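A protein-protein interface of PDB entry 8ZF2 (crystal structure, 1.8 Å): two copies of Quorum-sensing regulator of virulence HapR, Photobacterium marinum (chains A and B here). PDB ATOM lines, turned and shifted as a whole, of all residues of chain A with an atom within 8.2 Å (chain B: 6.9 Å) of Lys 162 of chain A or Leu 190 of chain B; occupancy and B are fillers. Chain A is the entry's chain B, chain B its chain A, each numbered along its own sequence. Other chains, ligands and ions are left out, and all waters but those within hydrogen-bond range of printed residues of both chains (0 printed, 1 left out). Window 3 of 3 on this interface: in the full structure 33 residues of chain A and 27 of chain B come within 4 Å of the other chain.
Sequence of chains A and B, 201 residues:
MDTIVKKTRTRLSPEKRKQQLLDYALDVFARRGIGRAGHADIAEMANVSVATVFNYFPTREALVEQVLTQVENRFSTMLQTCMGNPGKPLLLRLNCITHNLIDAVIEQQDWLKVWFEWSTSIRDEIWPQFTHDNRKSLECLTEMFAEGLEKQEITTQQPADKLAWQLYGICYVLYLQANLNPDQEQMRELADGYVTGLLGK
NE2 of Gln 177 of chain B lies close to NE1 of Trp 165 of chain A (3.2 Å).
OH of Tyr 194 of chain B lies within hydrogen-bond range of OE1 of Gln 177 of chain B, 2.9 Å away.
Among the printed residues, merely in contact across the chains: Lys 162 of chain A with Leu 190 of chain B (3.7 Å), Trp 165 of chain A with Val 173 of chain B (3.2 Å), Trp 165 of chain A with Tyr 194 of chain B (3.4 Å), Gln 166 of chain A with Tyr 194 of chain B (3.5 Å) and Gly 169 of chain A with Val 173 of chain B (3.3 Å).
Of the printed residues of chain A, Val 173 of chain B touches Trp 165 and Gly 169. Printed residues of chain A within 4 Å of Gln 177 of chain B: Trp 165 (3.2 Å). Leu 190 of chain B touches one residue of chain A. No residue of chain A comes within 4 Å of Ala 191 of chain B. Gly 193 of chain B touches none of the printed residues of chain A. The nearest residue of chain B that does not touch Lys 162 of chain A is Tyr 194 of chain B (4.03 Å).
Printed residues of chain B that touch a printed residue of chain A: Val 173, Gln 177, Leu 190 and Tyr 194. Of the 18 printed residues of chain A, 4 touch a printed residue of chain B. Printed residues of chain A that touch a printed residue of chain B: Lys 162, Trp 165, Gln 166 and Gly 169. Among the printed residues, no Asp or Glu carboxylate lies within 4 Å of a Lys or Arg side-chain nitrogen of the other chain.
No position is printed for both chains.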
ATOM      1  N   LEU A 138       6.800   5.225 -16.233  1.00  0.00           N
ATOM      2  CA  LEU A 138       8.224   5.010 -16.452  1.00  0.00           C
ATOM      3  C   LEU A 138       8.898   4.501 -15.184  1.00  0.00           C
ATOM      4  O   LEU A 138       9.716   3.572 -15.233  1.00  0.00           O
ATOM      5  CB  LEU A 138       8.878   6.308 -16.924  1.00  0.00           C
ATOM      6  CG  LEU A 138      10.389   6.260 -17.162  1.00  0.00           C
ATOM      7  CD1 LEU A 138      10.748   5.234 -18.219  1.00  0.00           C
ATOM      8  CD2 LEU A 138      10.922   7.639 -17.538  1.00  0.00           C
ATOM      9  N   LEU A 141       7.869   0.807 -14.647  1.00  0.00           N
ATOM     10  CA  LEU A 141       8.646  -0.098 -15.487  1.00  0.00           C
ATOM     11  C   LEU A 141      10.093  -0.184 -15.018  1.00  0.00           C
ATOM     12  O   LEU A 141      10.706  -1.257 -15.072  1.00  0.00           O
ATOM     13  CB  LEU A 141       8.585   0.356 -16.943  1.00  0.00           C
ATOM     14  CG  LEU A 141       7.211   0.332 -17.607  1.00  0.00           C
ATOM     15  CD1 LEU A 141       7.306   0.974 -18.988  1.00  0.00           C
ATOM     16  CD2 LEU A 141       6.685  -1.105 -17.698  1.00  0.00           C
ATOM     17  N   THR A 142      10.656   0.936 -14.559  1.00  0.00           N
ATOM     18  CA  THR A 142      12.034   0.931 -14.075  1.00  0.00           C
ATOM     19  C   THR A 142      12.179   0.027 -12.856  1.00  0.00           C
ATOM     20  O   THR A 142      13.117  -0.773 -12.775  1.00  0.00           O
ATOM     21  CB  THR A 142      12.492   2.356 -13.749  1.00  0.00           C
ATOM     22  OG1 THR A 142      12.446   3.170 -14.933  1.00  0.00           O
ATOM     23  CG2 THR A 142      13.911   2.342 -13.207  1.00  0.00           C
ATOM     24  N   PHE A 145      12.202  -3.630 -13.915  1.00  0.00           N
ATOM     25  CA  PHE A 145      13.479  -4.121 -14.427  1.00  0.00           C
ATOM     26  C   PHE A 145      14.528  -4.195 -13.325  1.00  0.00           C
ATOM     27  O   PHE A 145      15.345  -5.123 -13.302  1.00  0.00           O
ATOM     28  CB  PHE A 145      13.962  -3.248 -15.584  1.00  0.00           C
ATOM     29  CG  PHE A 145      13.326  -3.595 -16.897  1.00  0.00           C
ATOM     30  CD1 PHE A 145      13.599  -4.808 -17.510  1.00  0.00           C
ATOM     31  CD2 PHE A 145      12.445  -2.722 -17.511  1.00  0.00           C
ATOM     32  CE1 PHE A 145      13.011  -5.143 -18.712  1.00  0.00           C
ATOM     33  CE2 PHE A 145      11.854  -3.057 -18.715  1.00  0.00           C
ATOM     34  CZ  PHE A 145      12.133  -4.265 -19.314  1.00  0.00           C
ATOM     35  N   GLN A 157      23.800  -5.273 -17.875  1.00  0.00           N
ATOM     36  CA  GLN A 157      24.540  -4.570 -18.919  1.00  0.00           C
ATOM     37  C   GLN A 157      24.009  -3.161 -19.135  1.00  0.00           C
ATOM     38  O   GLN A 157      24.779  -2.246 -19.449  1.00  0.00           O
ATOM     39  CB  GLN A 157      24.468  -5.349 -20.233  1.00  0.00           C
ATOM     40  CG  GLN A 157      25.041  -6.751 -20.177  1.00  0.00           C
ATOM     41  CD  GLN A 157      25.061  -7.416 -21.539  1.00  0.00           C
ATOM     42  OE1 GLN A 157      25.957  -7.176 -22.350  1.00  0.00           O
ATOM     43  NE2 GLN A 157      24.045  -8.231 -21.812  1.00  0.00           N
ATOM     44  N   GLN A 158      22.697  -2.967 -18.983  1.00  0.00           N
ATOM     45  CA  GLN A 158      22.078  -1.665 -19.137  1.00  0.00           C
ATOM     46  C   GLN A 158      21.303  -1.291 -17.880  1.00  0.00           C
ATOM     47  O   GLN A 158      20.732  -2.166 -17.220  1.00  0.00           O
ATOM     48  CB  GLN A 158      21.139  -1.641 -20.358  1.00  0.00           C
ATOM     49  CG  GLN A 158      21.851  -1.951 -21.677  1.00  0.00           C
ATOM     50  CD  GLN A 158      20.995  -1.663 -22.903  1.00  0.00           C
ATOM     51  OE1 GLN A 158      20.184  -0.734 -22.908  1.00  0.00           O
ATOM     52  NE2 GLN A 158      21.180  -2.457 -23.955  1.00  0.00           N
ATOM     53  N   PRO A 159      21.283  -0.008 -17.511  1.00  0.00           N
ATOM     54  CA  PRO A 159      20.513   0.409 -16.333  1.00  0.00           C
ATOM     55  C   PRO A 159      19.030   0.113 -16.504  1.00  0.00           C
ATOM     56  O   PRO A 159      18.508   0.061 -17.620  1.00  0.00           O
ATOM     57  CB  PRO A 159      20.776   1.917 -16.254  1.00  0.00           C
ATOM     58  CG  PRO A 159      22.056   2.117 -16.995  1.00  0.00           C
ATOM     59  CD  PRO A 159      22.050   1.105 -18.095  1.00  0.00           C
ATOM     60  N   ALA A 160      18.352  -0.084 -15.368  1.00  0.00           N
ATOM     61  CA  ALA A 160      16.938  -0.449 -15.396  1.00  0.00           C
ATOM     62  C   ALA A 160      16.101   0.601 -16.114  1.00  0.00           C
ATOM     63  O   ALA A 160      15.146   0.261 -16.821  1.00  0.00           O
ATOM     64  CB  ALA A 160      16.421  -0.663 -13.974  1.00  0.00           C
ATOM     65  N   ASP A 161      16.441   1.883 -15.948  1.00  0.00           N
ATOM     66  CA  ASP A 161      15.688   2.934 -16.631  1.00  0.00           C
ATOM     67  C   ASP A 161      15.849   2.845 -18.143  1.00  0.00           C
ATOM     68  O   ASP A 161      14.912   3.160 -18.888  1.00  0.00           O
ATOM     69  CB  ASP A 161      16.134   4.311 -16.134  1.00  0.00           C
ATOM     70  CG  ASP A 161      15.262   5.433 -16.662  1.00  0.00           C
ATOM     71  OD1 ASP A 161      14.028   5.344 -16.502  1.00  0.00           O
ATOM     72  OD2 ASP A 161      15.807   6.412 -17.225  1.00  0.00           O
ATOM     73  N   LYS A 162      17.022   2.423 -18.615  1.00  0.00           N
ATOM     74  CA  LYS A 162      17.222   2.292 -20.051  1.00  0.00           C
ATOM     75  C   LYS A 162      16.442   1.112 -20.610  1.00  0.00           C
ATOM     76  O   LYS A 162      15.940   1.183 -21.738  1.00  0.00           O
ATOM     77  CB  LYS A 162      18.712   2.161 -20.378  1.00  0.00           C
ATOM     78  CG  LYS A 162      19.512   3.477 -20.370  1.00  0.00           C
ATOM     79  CD  LYS A 162      19.385   4.262 -19.063  1.00  0.00           C
ATOM     80  CE  LYS A 162      20.336   5.454 -19.019  1.00  0.00           C
ATOM     81  NZ  LYS A 162      21.765   5.058 -19.204  1.00  0.00           N
ATOM     82  N   LEU A 163      16.320   0.029 -19.840  1.00  0.00           N
ATOM     83  CA  LEU A 163      15.469  -1.080 -20.256  1.00  0.00           C
ATOM     84  C   LEU A 163      14.005  -0.663 -20.303  1.00  0.00           C
ATOM     85  O   LEU A 163      13.267  -1.065 -21.214  1.00  0.00           O
ATOM     86  CB  LEU A 163      15.667  -2.270 -19.313  1.00  0.00           C
ATOM     87  CG  LEU A 163      17.090  -2.835 -19.286  1.00  0.00           C
ATOM     88  CD1 LEU A 163      17.293  -3.756 -18.086  1.00  0.00           C
ATOM     89  CD2 LEU A 163      17.398  -3.571 -20.585  1.00  0.00           C
ATOM     90  N   ALA A 164      13.567   0.143 -19.332  1.00  0.00           N
ATOM     91  CA  ALA A 164      12.191   0.638 -19.333  1.00  0.00           C
ATOM     92  C   ALA A 164      11.889   1.416 -20.608  1.00  0.00           C
ATOM     93  O   ALA A 164      10.855   1.198 -21.250  1.00  0.00           O
ATOM     94  CB  ALA A 164      11.943   1.510 -18.100  1.00  0.00           C
ATOM     95  N   TRP A 165      12.787   2.328 -20.991  1.00  0.00           N
ATOM     96  CA  TRP A 165      12.616   3.065 -22.241  1.00  0.00           C
ATOM     97  C   TRP A 165      12.624   2.126 -23.441  1.00  0.00           C
ATOM     98  O   TRP A 165      11.852   2.309 -24.390  1.00  0.00           O
ATOM     99  CB  TRP A 165      13.719   4.113 -22.389  1.00  0.00           C
ATOM    100  CG  TRP A 165      13.477   5.377 -21.622  1.00  0.00           C
ATOM    101  CD1 TRP A 165      14.144   5.794 -20.510  1.00  0.00           C
ATOM    102  CD2 TRP A 165      12.511   6.395 -21.916  1.00  0.00           C
ATOM    103  NE1 TRP A 165      13.654   7.006 -20.089  1.00  0.00           N
ATOM    104  CE2 TRP A 165      12.649   7.397 -20.933  1.00  0.00           C
ATOM    105  CE3 TRP A 165      11.539   6.556 -22.910  1.00  0.00           C
ATOM    106  CZ2 TRP A 165      11.855   8.544 -20.915  1.00  0.00           C
ATOM    107  CZ3 TRP A 165      10.749   7.703 -22.890  1.00  0.00           C
ATOM    108  CH2 TRP A 165      10.911   8.676 -21.898  1.00  0.00           C
ATOM    109  N   GLN A 166      13.489   1.110 -23.414  1.00  0.00           N
ATOM    110  CA  GLN A 166      13.544   0.150 -24.514  1.00  0.00           C
ATOM    111  C   GLN A 166      12.221  -0.592 -24.668  1.00  0.00           C
ATOM    112  O   GLN A 166      11.742  -0.798 -25.788  1.00  0.00           O
ATOM    113  CB  GLN A 166      14.692  -0.830 -24.284  1.00  0.00           C
ATOM    114  CG  GLN A 166      16.063  -0.254 -24.612  1.00  0.00           C
ATOM    115  CD  GLN A 166      16.950  -1.245 -25.329  1.00  0.00           C
ATOM    116  OE1 GLN A 166      16.989  -2.428 -24.982  1.00  0.00           O
ATOM    117  NE2 GLN A 166      17.663  -0.770 -26.343  1.00  0.00           N
ATOM    118  N   LEU A 167      11.611  -0.989 -23.549  1.00  0.00           N
ATOM    119  CA  LEU A 167      10.316  -1.663 -23.603  1.00  0.00           C
ATOM    120  C   LEU A 167       9.245  -0.739 -24.165  1.00  0.00           C
ATOM    121  O   LEU A 167       8.332  -1.178 -24.877  1.00  0.00           O
ATOM    122  CB  LEU A 167       9.928  -2.144 -22.206  1.00  0.00           C
ATOM    123  CG  LEU A 167       8.524  -2.729 -22.075  1.00  0.00           C
ATOM    124  CD1 LEU A 167       8.426  -4.006 -22.895  1.00  0.00           C
ATOM    125  CD2 LEU A 167       8.192  -2.985 -20.617  1.00  0.00           C
ATOM    126  N   TYR A 168       9.338   0.547 -23.849  1.00  0.00           N
ATOM    127  CA  TYR A 168       8.405   1.517 -24.402  1.00  0.00           C
ATOM    128  C   TYR A 168       8.513   1.588 -25.929  1.00  0.00           C
ATOM    129  O   TYR A 168       7.496   1.664 -26.629  1.00  0.00           O
ATOM    130  CB  TYR A 168       8.668   2.859 -23.722  1.00  0.00           C
ATOM    131  CG  TYR A 168       7.814   4.007 -24.155  1.00  0.00           C
ATOM    132  CD1 TYR A 168       6.524   3.811 -24.625  1.00  0.00           C
ATOM    133  CD2 TYR A 168       8.275   5.310 -24.026  1.00  0.00           C
ATOM    134  CE1 TYR A 168       5.737   4.883 -25.010  1.00  0.00           C
ATOM    135  CE2 TYR A 168       7.498   6.378 -24.390  1.00  0.00           C
ATOM    136  CZ  TYR A 168       6.229   6.164 -24.883  1.00  0.00           C
ATOM    137  OH  TYR A 168       5.455   7.244 -25.251  1.00  0.00           O
ATOM    138  N   GLY A 169       9.731   1.535 -26.468  1.00  0.00           N
ATOM    139  CA  GLY A 169       9.877   1.478 -27.917  1.00  0.00           C
ATOM    140  C   GLY A 169       9.299   0.202 -28.502  1.00  0.00           C
ATOM    141  O   GLY A 169       8.671   0.218 -29.566  1.00  0.00           O
ATOM    142  N   LEU A 198      14.873  -8.677 -25.684  1.00  0.00           N
ATOM    143  CA  LEU A 198      15.140  -7.758 -24.580  1.00  0.00           C
ATOM    144  C   LEU A 198      15.731  -8.485 -23.376  1.00  0.00           C
ATOM    145  O   LEU A 198      16.657  -7.983 -22.728  1.00  0.00           O
ATOM    146  CB  LEU A 198      13.846  -7.036 -24.193  1.00  0.00           C
ATOM    147  CG  LEU A 198      13.879  -6.029 -23.041  1.00  0.00           C
ATOM    148  CD1 LEU A 198      14.926  -4.944 -23.278  1.00  0.00           C
ATOM    149  CD2 LEU A 198      12.497  -5.418 -22.840  1.00  0.00           C
ATOM    150  N   ILE B 102      18.527  12.888 -33.403  1.00  0.00           N
ATOM    151  CA  ILE B 102      18.703  13.739 -32.228  1.00  0.00           C
ATOM    152  C   ILE B 102      18.840  15.198 -32.642  1.00  0.00           C
ATOM    153  O   ILE B 102      18.157  16.080 -32.107  1.00  0.00           O
ATOM    154  CB  ILE B 102      19.918  13.272 -31.408  1.00  0.00           C
ATOM    155  CG1 ILE B 102      19.612  11.949 -30.705  1.00  0.00           C
ATOM    156  CG2 ILE B 102      20.330  14.339 -30.402  1.00  0.00           C
ATOM    157  CD1 ILE B 102      20.841  11.261 -30.169  1.00  0.00           C
ATOM    158  N   ILE B 170      13.567   2.234 -31.192  1.00  0.00           N
ATOM    159  CA  ILE B 170      14.637   3.020 -30.576  1.00  0.00           C
ATOM    160  C   ILE B 170      14.560   4.475 -31.030  1.00  0.00           C
ATOM    161  O   ILE B 170      14.755   5.403 -30.233  1.00  0.00           O
ATOM    162  CB  ILE B 170      16.008   2.396 -30.898  1.00  0.00           C
ATOM    163  CG1 ILE B 170      16.183   1.071 -30.147  1.00  0.00           C
ATOM    164  CG2 ILE B 170      17.144   3.367 -30.571  1.00  0.00           C
ATOM    165  CD1 ILE B 170      17.361   0.242 -30.619  1.00  0.00           C
ATOM    166  N   VAL B 173      11.787   6.243 -29.008  1.00  0.00           N
ATOM    167  CA  VAL B 173      12.104   6.631 -27.634  1.00  0.00           C
ATOM    168  C   VAL B 173      13.181   7.711 -27.615  1.00  0.00           C
ATOM    169  O   VAL B 173      13.146   8.625 -26.781  1.00  0.00           O
ATOM    170  CB  VAL B 173      12.497   5.408 -26.784  1.00  0.00           C
ATOM    171  CG1 VAL B 173      11.306   4.486 -26.624  1.00  0.00           C
ATOM    172  CG2 VAL B 173      13.677   4.671 -27.375  1.00  0.00           C
ATOM    173  N   LEU B 174      14.145   7.639 -28.537  1.00  0.00           N
ATOM    174  CA  LEU B 174      15.123   8.718 -28.652  1.00  0.00           C
ATOM    175  C   LEU B 174      14.434  10.034 -28.989  1.00  0.00           C
ATOM    176  O   LEU B 174      14.806  11.093 -28.470  1.00  0.00           O
ATOM    177  CB  LEU B 174      16.173   8.380 -29.716  1.00  0.00           C
ATOM    178  CG  LEU B 174      17.306   7.424 -29.348  1.00  0.00           C
ATOM    179  CD1 LEU B 174      18.194   7.156 -30.563  1.00  0.00           C
ATOM    180  CD2 LEU B 174      18.138   7.966 -28.185  1.00  0.00           C
ATOM    181  N   GLN B 177      12.816  11.238 -25.803  1.00  0.00           N
ATOM    182  CA  GLN B 177      13.795  11.621 -24.789  1.00  0.00           C
ATOM    183  C   GLN B 177      14.536  12.888 -25.179  1.00  0.00           C
ATOM    184  O   GLN B 177      14.873  13.698 -24.310  1.00  0.00           O
ATOM    185  CB  GLN B 177      14.788  10.488 -24.539  1.00  0.00           C
ATOM    186  CG  GLN B 177      14.200   9.297 -23.787  1.00  0.00           C
ATOM    187  CD  GLN B 177      15.218   8.199 -23.586  1.00  0.00           C
ATOM    188  OE1 GLN B 177      15.582   7.497 -24.530  1.00  0.00           O
ATOM    189  NE2 GLN B 177      15.700   8.055 -22.356  1.00  0.00           N
ATOM    190  N   ALA B 178      14.789  13.077 -26.475  1.00  0.00           N
ATOM    191  CA  ALA B 178      15.463  14.288 -26.925  1.00  0.00           C
ATOM    192  C   ALA B 178      14.547  15.500 -26.843  1.00  0.00           C
ATOM    193  O   ALA B 178      15.015  16.612 -26.577  1.00  0.00           O
ATOM    194  CB  ALA B 178      15.978  14.098 -28.349  1.00  0.00           C
ATOM    195  N   ASN B 181      14.821  16.370 -23.284  1.00  0.00           N
ATOM    196  CA  ASN B 181      16.137  16.911 -22.948  1.00  0.00           C
ATOM    197  C   ASN B 181      16.938  17.108 -24.227  1.00  0.00           C
ATOM    198  O   ASN B 181      17.734  16.245 -24.619  1.00  0.00           O
ATOM    199  CB  ASN B 181      16.883  15.992 -21.978  1.00  0.00           C
ATOM    200  CG  ASN B 181      18.286  16.480 -21.676  1.00  0.00           C
ATOM    201  OD1 ASN B 181      18.517  17.680 -21.548  1.00  0.00           O
ATOM    202  ND2 ASN B 181      19.232  15.551 -21.567  1.00  0.00           N
ATOM    203  N   GLN B 184      22.681  17.542 -26.926  1.00  0.00           N
ATOM    204  CA  GLN B 184      23.284  16.635 -27.899  1.00  0.00           C
ATOM    205  C   GLN B 184      24.178  15.600 -27.229  1.00  0.00           C
ATOM    206  O   GLN B 184      24.091  14.405 -27.534  1.00  0.00           O
ATOM    207  CB  GLN B 184      24.079  17.419 -28.942  1.00  0.00           C
ATOM    208  CG  GLN B 184      24.644  16.509 -30.021  1.00  0.00           C
ATOM    209  CD  GLN B 184      25.543  17.230 -30.996  1.00  0.00           C
ATOM    210  OE1 GLN B 184      25.092  17.715 -32.036  1.00  0.00           O
ATOM    211  NE2 GLN B 184      26.829  17.300 -30.669  1.00  0.00           N
ATOM    212  N   GLU B 185      25.058  16.036 -26.322  1.00  0.00           N
ATOM    213  CA  GLU B 185      26.002  15.096 -25.725  1.00  0.00           C
ATOM    214  C   GLU B 185      25.280  14.038 -24.899  1.00  0.00           C
ATOM    215  O   GLU B 185      25.569  12.841 -25.011  1.00  0.00           O
ATOM    216  CB  GLU B 185      27.030  15.834 -24.866  1.00  0.00           C
ATOM    217  CG  GLU B 185      27.958  14.882 -24.118  1.00  0.00           C
ATOM    218  CD  GLU B 185      28.973  15.601 -23.255  1.00  0.00           C
ATOM    219  OE1 GLU B 185      29.366  16.732 -23.609  1.00  0.00           O
ATOM    220  OE2 GLU B 185      29.375  15.032 -22.217  1.00  0.00           O
ATOM    221  N   GLN B 186      24.334  14.462 -24.059  1.00  0.00           N
ATOM    222  CA  GLN B 186      23.604  13.493 -23.247  1.00  0.00           C
ATOM    223  C   GLN B 186      22.764  12.570 -24.122  1.00  0.00           C
ATOM    224  O   GLN B 186      22.634  11.375 -23.832  1.00  0.00           O
ATOM    225  CB  GLN B 186      22.732  14.215 -22.219  1.00  0.00           C
ATOM    226  CG  GLN B 186      23.529  14.919 -21.118  1.00  0.00           C
ATOM    227  CD  GLN B 186      22.661  15.739 -20.179  1.00  0.00           C
ATOM    228  OE1 GLN B 186      21.455  15.882 -20.387  1.00  0.00           O
ATOM    229  NE2 GLN B 186      23.275  16.280 -19.132  1.00  0.00           N
ATOM    230  N   MET B 187      22.209  13.100 -25.214  1.00  0.00           N
ATOM    231  CA  MET B 187      21.320  12.300 -26.047  1.00  0.00           C
ATOM    232  C   MET B 187      22.128  11.303 -26.872  1.00  0.00           C
ATOM    233  O   MET B 187      21.704  10.160 -27.077  1.00  0.00           O
ATOM    234  CB  MET B 187      20.509  13.222 -26.960  1.00  0.00           C
ATOM    235  CG  MET B 187      19.137  13.650 -26.422  1.00  0.00           C
ATOM    236  SD  MET B 187      18.186  12.550 -25.355  1.00  0.00           S
ATOM    237  CE  MET B 187      18.116  11.048 -26.319  1.00  0.00           C
ATOM    238  N   ARG B 188      23.306  11.720 -27.343  1.00  0.00           N
ATOM    239  CA  ARG B 188      24.172  10.812 -28.086  1.00  0.00           C
ATOM    240  C   ARG B 188      24.705   9.693 -27.199  1.00  0.00           C
ATOM    241  O   ARG B 188      24.888   8.567 -27.669  1.00  0.00           O
ATOM    242  CB  ARG B 188      25.320  11.598 -28.719  1.00  0.00           C
ATOM    243  CG  ARG B 188      24.910  12.398 -29.954  1.00  0.00           C
ATOM    244  CD  ARG B 188      26.129  12.977 -30.674  1.00  0.00           C
ATOM    245  NE  ARG B 188      25.751  13.777 -31.834  1.00  0.00           N
ATOM    246  CZ  ARG B 188      26.609  14.241 -32.734  1.00  0.00           C
ATOM    247  NH1 ARG B 188      27.908  14.007 -32.636  1.00  0.00           N
ATOM    248  NH2 ARG B 188      26.151  14.955 -33.759  1.00  0.00           N
ATOM    249  N   GLU B 189      24.955   9.969 -25.918  1.00  0.00           N
ATOM    250  CA  GLU B 189      25.323   8.891 -25.007  1.00  0.00           C
ATOM    251  C   GLU B 189      24.205   7.858 -24.898  1.00  0.00           C
ATOM    252  O   GLU B 189      24.461   6.649 -24.923  1.00  0.00           O
ATOM    253  CB  GLU B 189      25.670   9.457 -23.632  1.00  0.00           C
ATOM    254  CG  GLU B 189      25.954   8.393 -22.595  1.00  0.00           C
ATOM    255  CD  GLU B 189      26.671   8.940 -21.379  1.00  0.00           C
ATOM    256  OE1 GLU B 189      27.456   9.901 -21.528  1.00  0.00           O
ATOM    257  OE2 GLU B 189      26.451   8.408 -20.272  1.00  0.00           O
ATOM    258  N   LEU B 190      22.958   8.318 -24.783  1.00  0.00           N
ATOM    259  CA  LEU B 190      21.825   7.398 -24.738  1.00  0.00           C
ATOM    260  C   LEU B 190      21.718   6.604 -26.032  1.00  0.00           C
ATOM    261  O   LEU B 190      21.505   5.386 -26.012  1.00  0.00           O
ATOM    262  CB  LEU B 190      20.530   8.169 -24.486  1.00  0.00           C
ATOM    263  CG  LEU B 190      20.232   8.691 -23.079  1.00  0.00           C
ATOM    264  CD1 LEU B 190      18.834   9.269 -23.039  1.00  0.00           C
ATOM    265  CD2 LEU B 190      20.367   7.579 -22.053  1.00  0.00           C
ATOM    266  N   ALA B 191      21.848   7.288 -27.171  1.00  0.00           N
ATOM    267  CA  ALA B 191      21.709   6.623 -28.464  1.00  0.00           C
ATOM    268  C   ALA B 191      22.821   5.606 -28.687  1.00  0.00           C
ATOM    269  O   ALA B 191      22.569   4.498 -29.175  1.00  0.00           O
ATOM    270  CB  ALA B 191      21.690   7.663 -29.586  1.00  0.00           C
ATOM    271  N   ASP B 192      24.059   5.959 -28.330  1.00  0.00           N
ATOM    272  CA  ASP B 192      25.155   5.008 -28.466  1.00  0.00           C
ATOM    273  C   ASP B 192      24.947   3.784 -27.580  1.00  0.00           C
ATOM    274  O   ASP B 192      25.311   2.671 -27.968  1.00  0.00           O
ATOM    275  CB  ASP B 192      26.489   5.695 -28.156  1.00  0.00           C
ATOM    276  CG  ASP B 192      26.781   6.862 -29.096  1.00  0.00           C
ATOM    277  OD1 ASP B 192      27.884   7.442 -28.997  1.00  0.00           O
ATOM    278  OD2 ASP B 192      25.928   7.184 -29.956  1.00  0.00           O
ATOM    279  N   GLY B 193      24.344   3.964 -26.403  1.00  0.00           N
ATOM    280  CA  GLY B 193      24.042   2.818 -25.561  1.00  0.00           C
ATOM    281  C   GLY B 193      23.024   1.887 -26.192  1.00  0.00           C
ATOM    282  O   GLY B 193      23.179   0.664 -26.152  1.00  0.00           O
ATOM    283  N   TYR B 194      21.969   2.455 -26.786  1.00  0.00           N
ATOM    284  CA  TYR B 194      20.970   1.641 -27.478  1.00  0.00           C
ATOM    285  C   TYR B 194      21.577   0.904 -28.666  1.00  0.00           C
ATOM    286  O   TYR B 194      21.278  -0.273 -28.894  1.00  0.00           O
ATOM    287  CB  TYR B 194      19.813   2.521 -27.957  1.00  0.00           C
ATOM    288  CG  TYR B 194      18.976   3.151 -26.862  1.00  0.00           C
ATOM    289  CD1 TYR B 194      18.737   2.490 -25.664  1.00  0.00           C
ATOM    290  CD2 TYR B 194      18.427   4.418 -27.035  1.00  0.00           C
ATOM    291  CE1 TYR B 194      17.965   3.073 -24.663  1.00  0.00           C
ATOM    292  CE2 TYR B 194      17.657   5.007 -26.044  1.00  0.00           C
ATOM    293  CZ  TYR B 194      17.429   4.332 -24.864  1.00  0.00           C
ATOM    294  OH  TYR B 194      16.663   4.925 -23.884  1.00  0.00           O
ATOM    295  N   VAL B 195      22.407   1.592 -29.451  1.00  0.00           N
ATOM    296  CA  VAL B 195      23.007   0.977 -30.631  1.00  0.00           C
ATOM    297  C   VAL B 195      23.981  -0.120 -30.228  1.00  0.00           C
ATOM    298  O   VAL B 195      24.019  -1.193 -30.846  1.00  0.00           O
ATOM    299  CB  VAL B 195      23.687   2.049 -31.501  1.00  0.00           C
ATOM    300  CG1 VAL B 195      24.609   1.410 -32.529  1.00  0.00           C
ATOM    301  CG2 VAL B 195      22.637   2.897 -32.184  1.00  0.00           C
